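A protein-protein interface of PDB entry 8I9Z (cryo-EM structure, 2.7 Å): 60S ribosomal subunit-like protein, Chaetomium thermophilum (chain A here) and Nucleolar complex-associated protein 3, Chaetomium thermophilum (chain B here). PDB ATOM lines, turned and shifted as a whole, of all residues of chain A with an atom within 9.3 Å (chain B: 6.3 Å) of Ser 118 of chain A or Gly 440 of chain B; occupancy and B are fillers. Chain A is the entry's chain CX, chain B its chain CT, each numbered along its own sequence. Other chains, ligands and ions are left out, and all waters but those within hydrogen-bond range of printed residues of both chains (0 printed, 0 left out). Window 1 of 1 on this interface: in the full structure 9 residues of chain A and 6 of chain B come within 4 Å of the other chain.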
ATOM      1  N   GLY A 114       9.330 -15.198 -18.448  1.00  0.00           N
ATOM      2  CA  GLY A 114      10.093 -14.020 -18.073  1.00  0.00           C
ATOM      3  C   GLY A 114       9.206 -12.903 -17.582  1.00  0.00           C
ATOM      4  O   GLY A 114       8.245 -13.131 -16.842  1.00  0.00           O
ATOM      5  N   GLN A 115       9.528 -11.681 -17.995  1.00  0.00           N
ATOM      6  CA  GLN A 115       8.885 -10.494 -17.445  1.00  0.00           C
ATOM      7  C   GLN A 115       7.533 -10.261 -18.105  1.00  0.00           C
ATOM      8  O   GLN A 115       7.432 -10.203 -19.335  1.00  0.00           O
ATOM      9  CB  GLN A 115       9.787  -9.279 -17.637  1.00  0.00           C
ATOM     10  CG  GLN A 115      10.645  -8.951 -16.426  1.00  0.00           C
ATOM     11  CD  GLN A 115      11.907  -9.789 -16.364  1.00  0.00           C
ATOM     12  OE1 GLN A 115      12.795  -9.658 -17.207  1.00  0.00           O
ATOM     13  NE2 GLN A 115      11.991 -10.657 -15.363  1.00  0.00           N
ATOM     14  N   ILE A 116       6.496 -10.118 -17.285  1.00  0.00           N
ATOM     15  CA  ILE A 116       5.157  -9.773 -17.741  1.00  0.00           C
ATOM     16  C   ILE A 116       4.816  -8.409 -17.164  1.00  0.00           C
ATOM     17  O   ILE A 116       4.993  -8.177 -15.963  1.00  0.00           O
ATOM     18  CB  ILE A 116       4.111 -10.818 -17.328  1.00  0.00           C
ATOM     19  CG1 ILE A 116       4.675 -12.231 -17.458  1.00  0.00           C
ATOM     20  CG2 ILE A 116       2.860 -10.665 -18.164  1.00  0.00           C
ATOM     21  CD1 ILE A 116       3.857 -13.275 -16.742  1.00  0.00           C
ATOM     22  N   GLU A 117       4.339  -7.508 -18.022  1.00  0.00           N
ATOM     23  CA  GLU A 117       4.040  -6.146 -17.590  1.00  0.00           C
ATOM     24  C   GLU A 117       2.821  -6.109 -16.677  1.00  0.00           C
ATOM     25  O   GLU A 117       2.725  -5.260 -15.785  1.00  0.00           O
ATOM     26  CB  GLU A 117       3.828  -5.248 -18.805  1.00  0.00           C
ATOM     27  CG  GLU A 117       4.890  -5.394 -19.874  1.00  0.00           C
ATOM     28  CD  GLU A 117       5.426  -4.059 -20.339  1.00  0.00           C
ATOM     29  OE1 GLU A 117       5.117  -3.038 -19.692  1.00  0.00           O
ATOM     30  OE2 GLU A 117       6.157  -4.031 -21.350  1.00  0.00           O
ATOM     31  N   SER A 118       1.876  -7.015 -16.893  1.00  0.00           N
ATOM     32  CA  SER A 118       0.655  -7.021 -16.102  1.00  0.00           C
ATOM     33  C   SER A 118       0.922  -7.548 -14.698  1.00  0.00           C
ATOM     34  O   SER A 118       1.546  -8.598 -14.528  1.00  0.00           O
ATOM     35  CB  SER A 118      -0.398  -7.878 -16.797  1.00  0.00           C
ATOM     36  OG  SER A 118      -0.585  -7.461 -18.137  1.00  0.00           O
ATOM     37  N   LYS A 119       0.447  -6.815 -13.688  1.00  0.00           N
ATOM     38  CA  LYS A 119       0.593  -7.279 -12.310  1.00  0.00           C
ATOM     39  C   LYS A 119      -0.304  -8.474 -12.017  1.00  0.00           C
ATOM     40  O   LYS A 119       0.078  -9.360 -11.245  1.00  0.00           O
ATOM     41  CB  LYS A 119       0.319  -6.158 -11.298  1.00  0.00           C
ATOM     42  CG  LYS A 119       1.235  -4.917 -11.300  1.00  0.00           C
ATOM     43  CD  LYS A 119       1.073  -3.924 -12.445  1.00  0.00           C
ATOM     44  CE  LYS A 119       2.443  -3.409 -12.869  1.00  0.00           C
ATOM     45  NZ  LYS A 119       2.453  -2.754 -14.198  1.00  0.00           N
ATOM     46  N   ILE A 120      -1.500  -8.518 -12.605  1.00  0.00           N
ATOM     47  CA  ILE A 120      -2.381  -9.655 -12.358  1.00  0.00           C
ATOM     48  C   ILE A 120      -1.848 -10.912 -13.031  1.00  0.00           C
ATOM     49  O   ILE A 120      -1.832 -11.987 -12.422  1.00  0.00           O
ATOM     50  CB  ILE A 120      -3.825  -9.340 -12.789  1.00  0.00           C
ATOM     51  CG1 ILE A 120      -4.367  -8.144 -12.008  1.00  0.00           C
ATOM     52  CG2 ILE A 120      -4.723 -10.543 -12.570  1.00  0.00           C
ATOM     53  CD1 ILE A 120      -5.824  -7.849 -12.272  1.00  0.00           C
ATOM     54  N   MET A 121      -1.384 -10.807 -14.280  1.00  0.00           N
ATOM     55  CA  MET A 121      -0.844 -11.984 -14.956  1.00  0.00           C
ATOM     56  C   MET A 121       0.453 -12.451 -14.311  1.00  0.00           C
ATOM     57  O   MET A 121       0.768 -13.646 -14.335  1.00  0.00           O
ATOM     58  CB  MET A 121      -0.621 -11.704 -16.439  1.00  0.00           C
ATOM     59  CG  MET A 121      -1.847 -11.220 -17.184  1.00  0.00           C
ATOM     60  SD  MET A 121      -1.665 -11.238 -18.980  1.00  0.00           S
ATOM     61  CE  MET A 121      -0.283 -12.358 -19.189  1.00  0.00           C
ATOM     62  N   ARG A 122       1.220 -11.524 -13.736  1.00  0.00           N
ATOM     63  CA  ARG A 122       2.403 -11.911 -12.978  1.00  0.00           C
ATOM     64  C   ARG A 122       2.026 -12.657 -11.711  1.00  0.00           C
ATOM     65  O   ARG A 122       2.770 -13.535 -11.262  1.00  0.00           O
ATOM     66  CB  ARG A 122       3.232 -10.678 -12.645  1.00  0.00           C
ATOM     67  CG  ARG A 122       4.675 -10.963 -12.294  1.00  0.00           C
ATOM     68  CD  ARG A 122       5.189 -10.029 -11.180  1.00  0.00           C
ATOM     69  NE  ARG A 122       4.847  -8.605 -11.261  1.00  0.00           N
ATOM     70  CZ  ARG A 122       4.995  -7.794 -12.307  1.00  0.00           C
ATOM     71  NH1 ARG A 122       5.637  -8.169 -13.402  1.00  0.00           N
ATOM     72  NH2 ARG A 122       4.525  -6.554 -12.232  1.00  0.00           N
ATOM     73  N   ALA A 123       0.880 -12.326 -11.121  1.00  0.00           N
ATOM     74  CA  ALA A 123       0.419 -13.047  -9.943  1.00  0.00           C
ATOM     75  C   ALA A 123      -0.111 -14.427 -10.303  1.00  0.00           C
ATOM     76  O   ALA A 123       0.148 -15.396  -9.582  1.00  0.00           O
ATOM     77  CB  ALA A 123      -0.651 -12.237  -9.215  1.00  0.00           C
ATOM     78  N   ARG A 124      -0.848 -14.537 -11.411  1.00  0.00           N
ATOM     79  CA  ARG A 124      -1.380 -15.830 -11.830  1.00  0.00           C
ATOM     80  C   ARG A 124      -0.273 -16.788 -12.239  1.00  0.00           C
ATOM     81  O   ARG A 124      -0.445 -18.007 -12.152  1.00  0.00           O
ATOM     82  CB  ARG A 124      -2.365 -15.646 -12.981  1.00  0.00           C
ATOM     83  CG  ARG A 124      -3.504 -14.709 -12.669  1.00  0.00           C
ATOM     84  CD  ARG A 124      -4.563 -15.403 -11.860  1.00  0.00           C
ATOM     85  NE  ARG A 124      -5.147 -14.516 -10.864  1.00  0.00           N
ATOM     86  CZ  ARG A 124      -6.340 -13.953 -10.972  1.00  0.00           C
ATOM     87  NH1 ARG A 124      -7.101 -14.151 -12.033  1.00  0.00           N
ATOM     88  NH2 ARG A 124      -6.779 -13.172  -9.991  1.00  0.00           N
ATOM     89  N   GLN A 125       0.861 -16.257 -12.697  1.00  0.00           N
ATOM     90  CA  GLN A 125       2.008 -17.102 -12.997  1.00  0.00           C
ATOM     91  C   GLN A 125       2.589 -17.725 -11.737  1.00  0.00           C
ATOM     92  O   GLN A 125       3.124 -18.837 -11.783  1.00  0.00           O
ATOM     93  CB  GLN A 125       3.067 -16.287 -13.730  1.00  0.00           C
ATOM     94  CG  GLN A 125       4.012 -17.104 -14.562  1.00  0.00           C
ATOM     95  CD  GLN A 125       5.230 -16.315 -14.971  1.00  0.00           C
ATOM     96  OE1 GLN A 125       5.804 -15.580 -14.170  1.00  0.00           O
ATOM     97  NE2 GLN A 125       5.634 -16.458 -16.225  1.00  0.00           N
ATOM     98  N   GLN B 436      -1.006   0.526 -20.589  1.00  0.00           N
ATOM     99  CA  GLN B 436      -0.597  -0.719 -21.229  1.00  0.00           C
ATOM    100  C   GLN B 436      -0.600  -1.899 -20.272  1.00  0.00           C
ATOM    101  O   GLN B 436      -0.939  -3.019 -20.667  1.00  0.00           O
ATOM    102  CB  GLN B 436       0.800  -0.552 -21.831  1.00  0.00           C
ATOM    103  CG  GLN B 436       1.281  -1.726 -22.631  1.00  0.00           C
ATOM    104  CD  GLN B 436       2.486  -1.394 -23.464  1.00  0.00           C
ATOM    105  OE1 GLN B 436       2.939  -0.262 -23.474  1.00  0.00           O
ATOM    106  NE2 GLN B 436       3.013  -2.382 -24.172  1.00  0.00           N
ATOM    107  N   ASP B 437      -0.222  -1.666 -19.017  1.00  0.00           N
ATOM    108  CA  ASP B 437      -0.173  -2.738 -18.032  1.00  0.00           C
ATOM    109  C   ASP B 437      -1.559  -3.285 -17.728  1.00  0.00           C
ATOM    110  O   ASP B 437      -1.715  -4.471 -17.417  1.00  0.00           O
ATOM    111  CB  ASP B 437       0.471  -2.222 -16.751  1.00  0.00           C
ATOM    112  CG  ASP B 437       1.564  -1.216 -17.016  1.00  0.00           C
ATOM    113  OD1 ASP B 437       2.639  -1.614 -17.511  1.00  0.00           O
ATOM    114  OD2 ASP B 437       1.345  -0.021 -16.735  1.00  0.00           O
ATOM    115  N   PHE B 438      -2.577  -2.433 -17.808  1.00  0.00           N
ATOM    116  CA  PHE B 438      -3.931  -2.832 -17.457  1.00  0.00           C
ATOM    117  C   PHE B 438      -4.627  -3.600 -18.569  1.00  0.00           C
ATOM    118  O   PHE B 438      -5.742  -4.083 -18.351  1.00  0.00           O
ATOM    119  CB  PHE B 438      -4.757  -1.602 -17.091  1.00  0.00           C
ATOM    120  CG  PHE B 438      -4.226  -0.839 -15.915  1.00  0.00           C
ATOM    121  CD1 PHE B 438      -3.537  -1.481 -14.902  1.00  0.00           C
ATOM    122  CD2 PHE B 438      -4.399   0.530 -15.834  1.00  0.00           C
ATOM    123  CE1 PHE B 438      -3.042  -0.774 -13.825  1.00  0.00           C
ATOM    124  CE2 PHE B 438      -3.907   1.244 -14.758  1.00  0.00           C
ATOM    125  CZ  PHE B 438      -3.227   0.591 -13.753  1.00  0.00           C
ATOM    126  N   PHE B 439      -4.018  -3.709 -19.750  1.00  0.00           N
ATOM    127  CA  PHE B 439      -4.648  -4.454 -20.833  1.00  0.00           C
ATOM    128  C   PHE B 439      -4.644  -5.948 -20.549  1.00  0.00           C
ATOM    129  O   PHE B 439      -5.622  -6.647 -20.838  1.00  0.00           O
ATOM    130  CB  PHE B 439      -3.952  -4.156 -22.155  1.00  0.00           C
ATOM    131  CG  PHE B 439      -4.868  -4.202 -23.334  1.00  0.00           C
ATOM    132  CD1 PHE B 439      -5.075  -5.383 -24.019  1.00  0.00           C
ATOM    133  CD2 PHE B 439      -5.536  -3.066 -23.748  1.00  0.00           C
ATOM    134  CE1 PHE B 439      -5.922  -5.424 -25.101  1.00  0.00           C
ATOM    135  CE2 PHE B 439      -6.383  -3.103 -24.827  1.00  0.00           C
ATOM    136  CZ  PHE B 439      -6.578  -4.282 -25.503  1.00  0.00           C
ATOM    137  N   GLY B 440      -3.550  -6.461 -19.991  1.00  0.00           N
ATOM    138  CA  GLY B 440      -3.518  -7.861 -19.618  1.00  0.00           C
ATOM    139  C   GLY B 440      -4.380  -8.167 -18.413  1.00  0.00           C
ATOM    140  O   GLY B 440      -4.812  -9.306 -18.226  1.00  0.00           O
ATOM    141  N   ASP B 441      -4.631  -7.161 -17.572  1.00  0.00           N
ATOM    142  CA  ASP B 441      -5.523  -7.344 -16.433  1.00  0.00           C
ATOM    143  C   ASP B 441      -6.964  -7.520 -16.887  1.00  0.00           C
ATOM    144  O   ASP B 441      -7.711  -8.322 -16.316  1.00  0.00           O
ATOM    145  CB  ASP B 441      -5.408  -6.156 -15.481  1.00  0.00           C
ATOM    146  CG  ASP B 441      -3.990  -5.917 -15.019  1.00  0.00           C
ATOM    147  OD1 ASP B 441      -3.064  -6.455 -15.654  1.00  0.00           O
ATOM    148  OD2 ASP B 441      -3.801  -5.195 -14.017  1.00  0.00           O
ATOM    149  N   LEU B 442      -7.377  -6.760 -17.901  1.00  0.00           N
ATOM    150  CA  LEU B 442      -8.727  -6.889 -18.436  1.00  0.00           C
ATOM    151  C   LEU B 442      -8.923  -8.248 -19.084  1.00  0.00           C
ATOM    152  O   LEU B 442      -9.998  -8.850 -18.987  1.00  0.00           O
ATOM    153  CB  LEU B 442      -8.999  -5.773 -19.442  1.00  0.00           C
ATOM    154  CG  LEU B 442      -9.065  -4.353 -18.894  1.00  0.00           C
ATOM    155  CD1 LEU B 442      -8.774  -3.354 -19.996  1.00  0.00           C
ATOM    156  CD2 LEU B 442     -10.424  -4.097 -18.290  1.00  0.00           C
ATOM    157  N   LEU B 443      -7.886  -8.749 -19.755  1.00  0.00           N
ATOM    158  CA  LEU B 443      -7.953 -10.075 -20.345  1.00  0.00           C
ATOM    159  C   LEU B 443      -7.969 -11.172 -19.290  1.00  0.00           C
ATOM    160  O   LEU B 443      -8.406 -12.289 -19.583  1.00  0.00           O
ATOM    161  CB  LEU B 443      -6.778 -10.275 -21.297  1.00  0.00           C
ATOM    162  CG  LEU B 443      -7.116 -11.075 -22.551  1.00  0.00           C
ATOM    163  CD1 LEU B 443      -7.900 -10.209 -23.515  1.00  0.00           C
ATOM    164  CD2 LEU B 443      -5.860 -11.610 -23.205  1.00  0.00           C
ATOM    165  N   GLU B 444      -7.508 -10.885 -18.072  1.00  0.00           N
ATOM    166  CA  GLU B 444      -7.549 -11.848 -16.982  1.00  0.00           C
ATOM    167  C   GLU B 444      -8.760 -11.691 -16.078  1.00  0.00           C
ATOM    168  O   GLU B 444      -9.153 -12.663 -15.427  1.00  0.00           O
ATOM    169  CB  GLU B 444      -6.280 -11.752 -16.131  1.00  0.00           C
ATOM    170  CG  GLU B 444      -5.164 -12.652 -16.605  1.00  0.00           C
ATOM    171  CD  GLU B 444      -5.117 -13.964 -15.855  1.00  0.00           C
ATOM    172  OE1 GLU B 444      -4.242 -14.798 -16.170  1.00  0.00           O
ATOM    173  OE2 GLU B 444      -5.954 -14.165 -14.952  1.00  0.00           O
ATOM    174  N   ALA B 445      -9.348 -10.498 -16.003  1.00  0.00           N
ATOM    175  CA  ALA B 445     -10.606 -10.348 -15.284  1.00  0.00           C
ATOM    176  C   ALA B 445     -11.750 -10.997 -16.044  1.00  0.00           C
ATOM    177  O   ALA B 445     -12.711 -11.478 -15.438  1.00  0.00           O
ATOM    178  CB  ALA B 445     -10.902  -8.869 -15.036  1.00  0.00           C
ATOM    179  N   LEU B 505       2.886  -7.594 -25.012  1.00  0.00           N
ATOM    180  CA  LEU B 505       1.897  -7.899 -23.989  1.00  0.00           C
ATOM    181  C   LEU B 505       1.431  -9.328 -24.209  1.00  0.00           C
ATOM    182  O   LEU B 505       0.784  -9.621 -25.218  1.00  0.00           O
ATOM    183  CB  LEU B 505       0.722  -6.932 -24.076  1.00  0.00           C
ATOM    184  CG  LEU B 505       0.923  -5.476 -23.683  1.00  0.00           C
ATOM    185  CD1 LEU B 505      -0.426  -4.885 -23.359  1.00  0.00           C
ATOM    186  CD2 LEU B 505       1.863  -5.364 -22.500  1.00  0.00           C
ATOM    187  N   HIS B 506       1.740 -10.218 -23.270  1.00  0.00           N
ATOM    188  CA  HIS B 506       1.490 -11.636 -23.496  1.00  0.00           C
ATOM    189  C   HIS B 506       0.002 -11.939 -23.422  1.00  0.00           C
ATOM    190  O   HIS B 506      -0.492 -12.457 -22.418  1.00  0.00           O
ATOM    191  CB  HIS B 506       2.269 -12.479 -22.490  1.00  0.00           C
ATOM    192  CG  HIS B 506       3.750 -12.295 -22.577  1.00  0.00           C
ATOM    193  ND1 HIS B 506       4.518 -11.917 -21.498  1.00  0.00           N
ATOM    194  CD2 HIS B 506       4.604 -12.428 -23.618  1.00  0.00           C
ATOM    195  CE1 HIS B 506       5.781 -11.828 -21.869  1.00  0.00           C
ATOM    196  NE2 HIS B 506       5.862 -12.135 -23.151  1.00  0.00           N
ATOM    197  N   LEU B 507      -0.712 -11.636 -24.498  1.00  0.00           N
ATOM    198  CA  LEU B 507      -2.163 -11.749 -24.554  1.00  0.00           C
ATOM    199  C   LEU B 507      -2.495 -13.000 -25.356  1.00  0.00           C
ATOM    200  O   LEU B 507      -2.549 -12.960 -26.589  1.00  0.00           O
ATOM    201  CB  LEU B 507      -2.777 -10.502 -25.182  1.00  0.00           C
ATOM    202  CG  LEU B 507      -2.435  -9.173 -24.507  1.00  0.00           C
ATOM    203  CD1 LEU B 507      -2.561  -8.034 -25.495  1.00  0.00           C
ATOM    204  CD2 LEU B 507      -3.307  -8.922 -23.294  1.00  0.00           C
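O of Gly 440 of chain B lies close to SD of Met 121 of chain A. OG of Ser 118 of chain A is in hydrogen-bond range of O of Asp 437 of chain B, 3.3 Å away. OD1 of Asp 437 of chain B is in salt-bridge range of NZ of Lys 119 of chain A (3.5 Å). The side-chain carboxylate (OE2) of Glu 444 of chain B lies within salt-bridge range of the guanidinium group (NH1) of Arg 124 of chain A, at 3.1 Å.
The backbone carbonyl oxygen (O) of Ile 116 of chain A is in hydrogen-bond range of the guanidinium group (NH1) of Arg 122 of chain A, at 2.6 Å. The backbone carbonyl oxygen of Glu 117 of chain A lies within hydrogen-bond range of the side-chain amino group of Lys 119 of chain A (3.0 Å).
Gln 115 of chain A touches His 506 of chain B (O to CE1, 3.4 Å). CG2 of Ile 116 of chain A touches ND1 of His 506 of chain B, 3.9 Å away. Glu 117 of chain A touches Asp 437 of chain B. OG of Ser 118 of chain A touches CA of Gly 440 of chain B (3.3 Å). Asp 441 of chain B touches Ser 118 of chain A (OD1 to CB, 3.2 Å). Ile 120 of chain A touches Asp 441 of chain B. Glu 444 of chain B touches Met 121 of chain A (CG to CG, 3.7 Å). His 506 of chain B touches Met 121 of chain A.
Ser 118 of chain A touches just these residues of chain B: Asp 437 (3.3 Å), Gly 440 (3.3 Å) and Asp 441 (3.2 Å). Gly 440 of chain B touches just these residues of chain A: Ser 118 (3.3 Å) and Met 121 (3.7 Å). Of chain A, only Ser 118 and Ile 120 come within 4 Å of Asp 441 of chain B. Of the printed residues of chain B, Gln 115 of chain A touches His 506 (3.4 Å). Printed residues of chain B within 4 Å of Ile 116 of chain A: His 506 (3.9 Å). Printed residues of chain B within 4 Å of Lys 119 of chain A: Asp 437 (3.3 Å). Printed residues of chain B within 4 Å of Arg 124 of chain A: Glu 444 (3.1 Å). Ala 445 of chain B touches none of the printed residues of chain A. Leu 505 of chain B touches none of the printed residues of chain A. The nearest residue of chain A that does not touch Gly 440 of chain B is Ile 120 of chain A (5.5 Å).
Of the 12 printed residues of chain A, 8 touch a printed residue of chain B. Printed residues of chain A that touch a printed residue of chain B: Gln 115, Ile 116, Glu 117, Ser 118, Lys 119, Ile 120, Met 121 and Arg 124. Hydrophobic or aromatic side chains of chain A within 4 Å of the printed part of chain B: Ile 116, Ile 120 and Met 121. Along chain A the printed residues that touch a printed residue of chain B span positions 115 to 124. Printed residues of chain B that touch a printed residue of chain A: Asp 437, Gly 440, Asp 441, Glu 444 and His 506. Hydrophobic or aromatic side chains of chain B within 4 Å of the printed part of chain A: His 506. Among the printed residues, Asp or Glu carboxylates within 4 Å of a Lys or Arg side-chain nitrogen of the other chain: Lys 119 of chain A with Asp 437 of chain B (3.5 Å) and Arg 124 of chain A with Glu 444 of chain B (3.1 Å).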
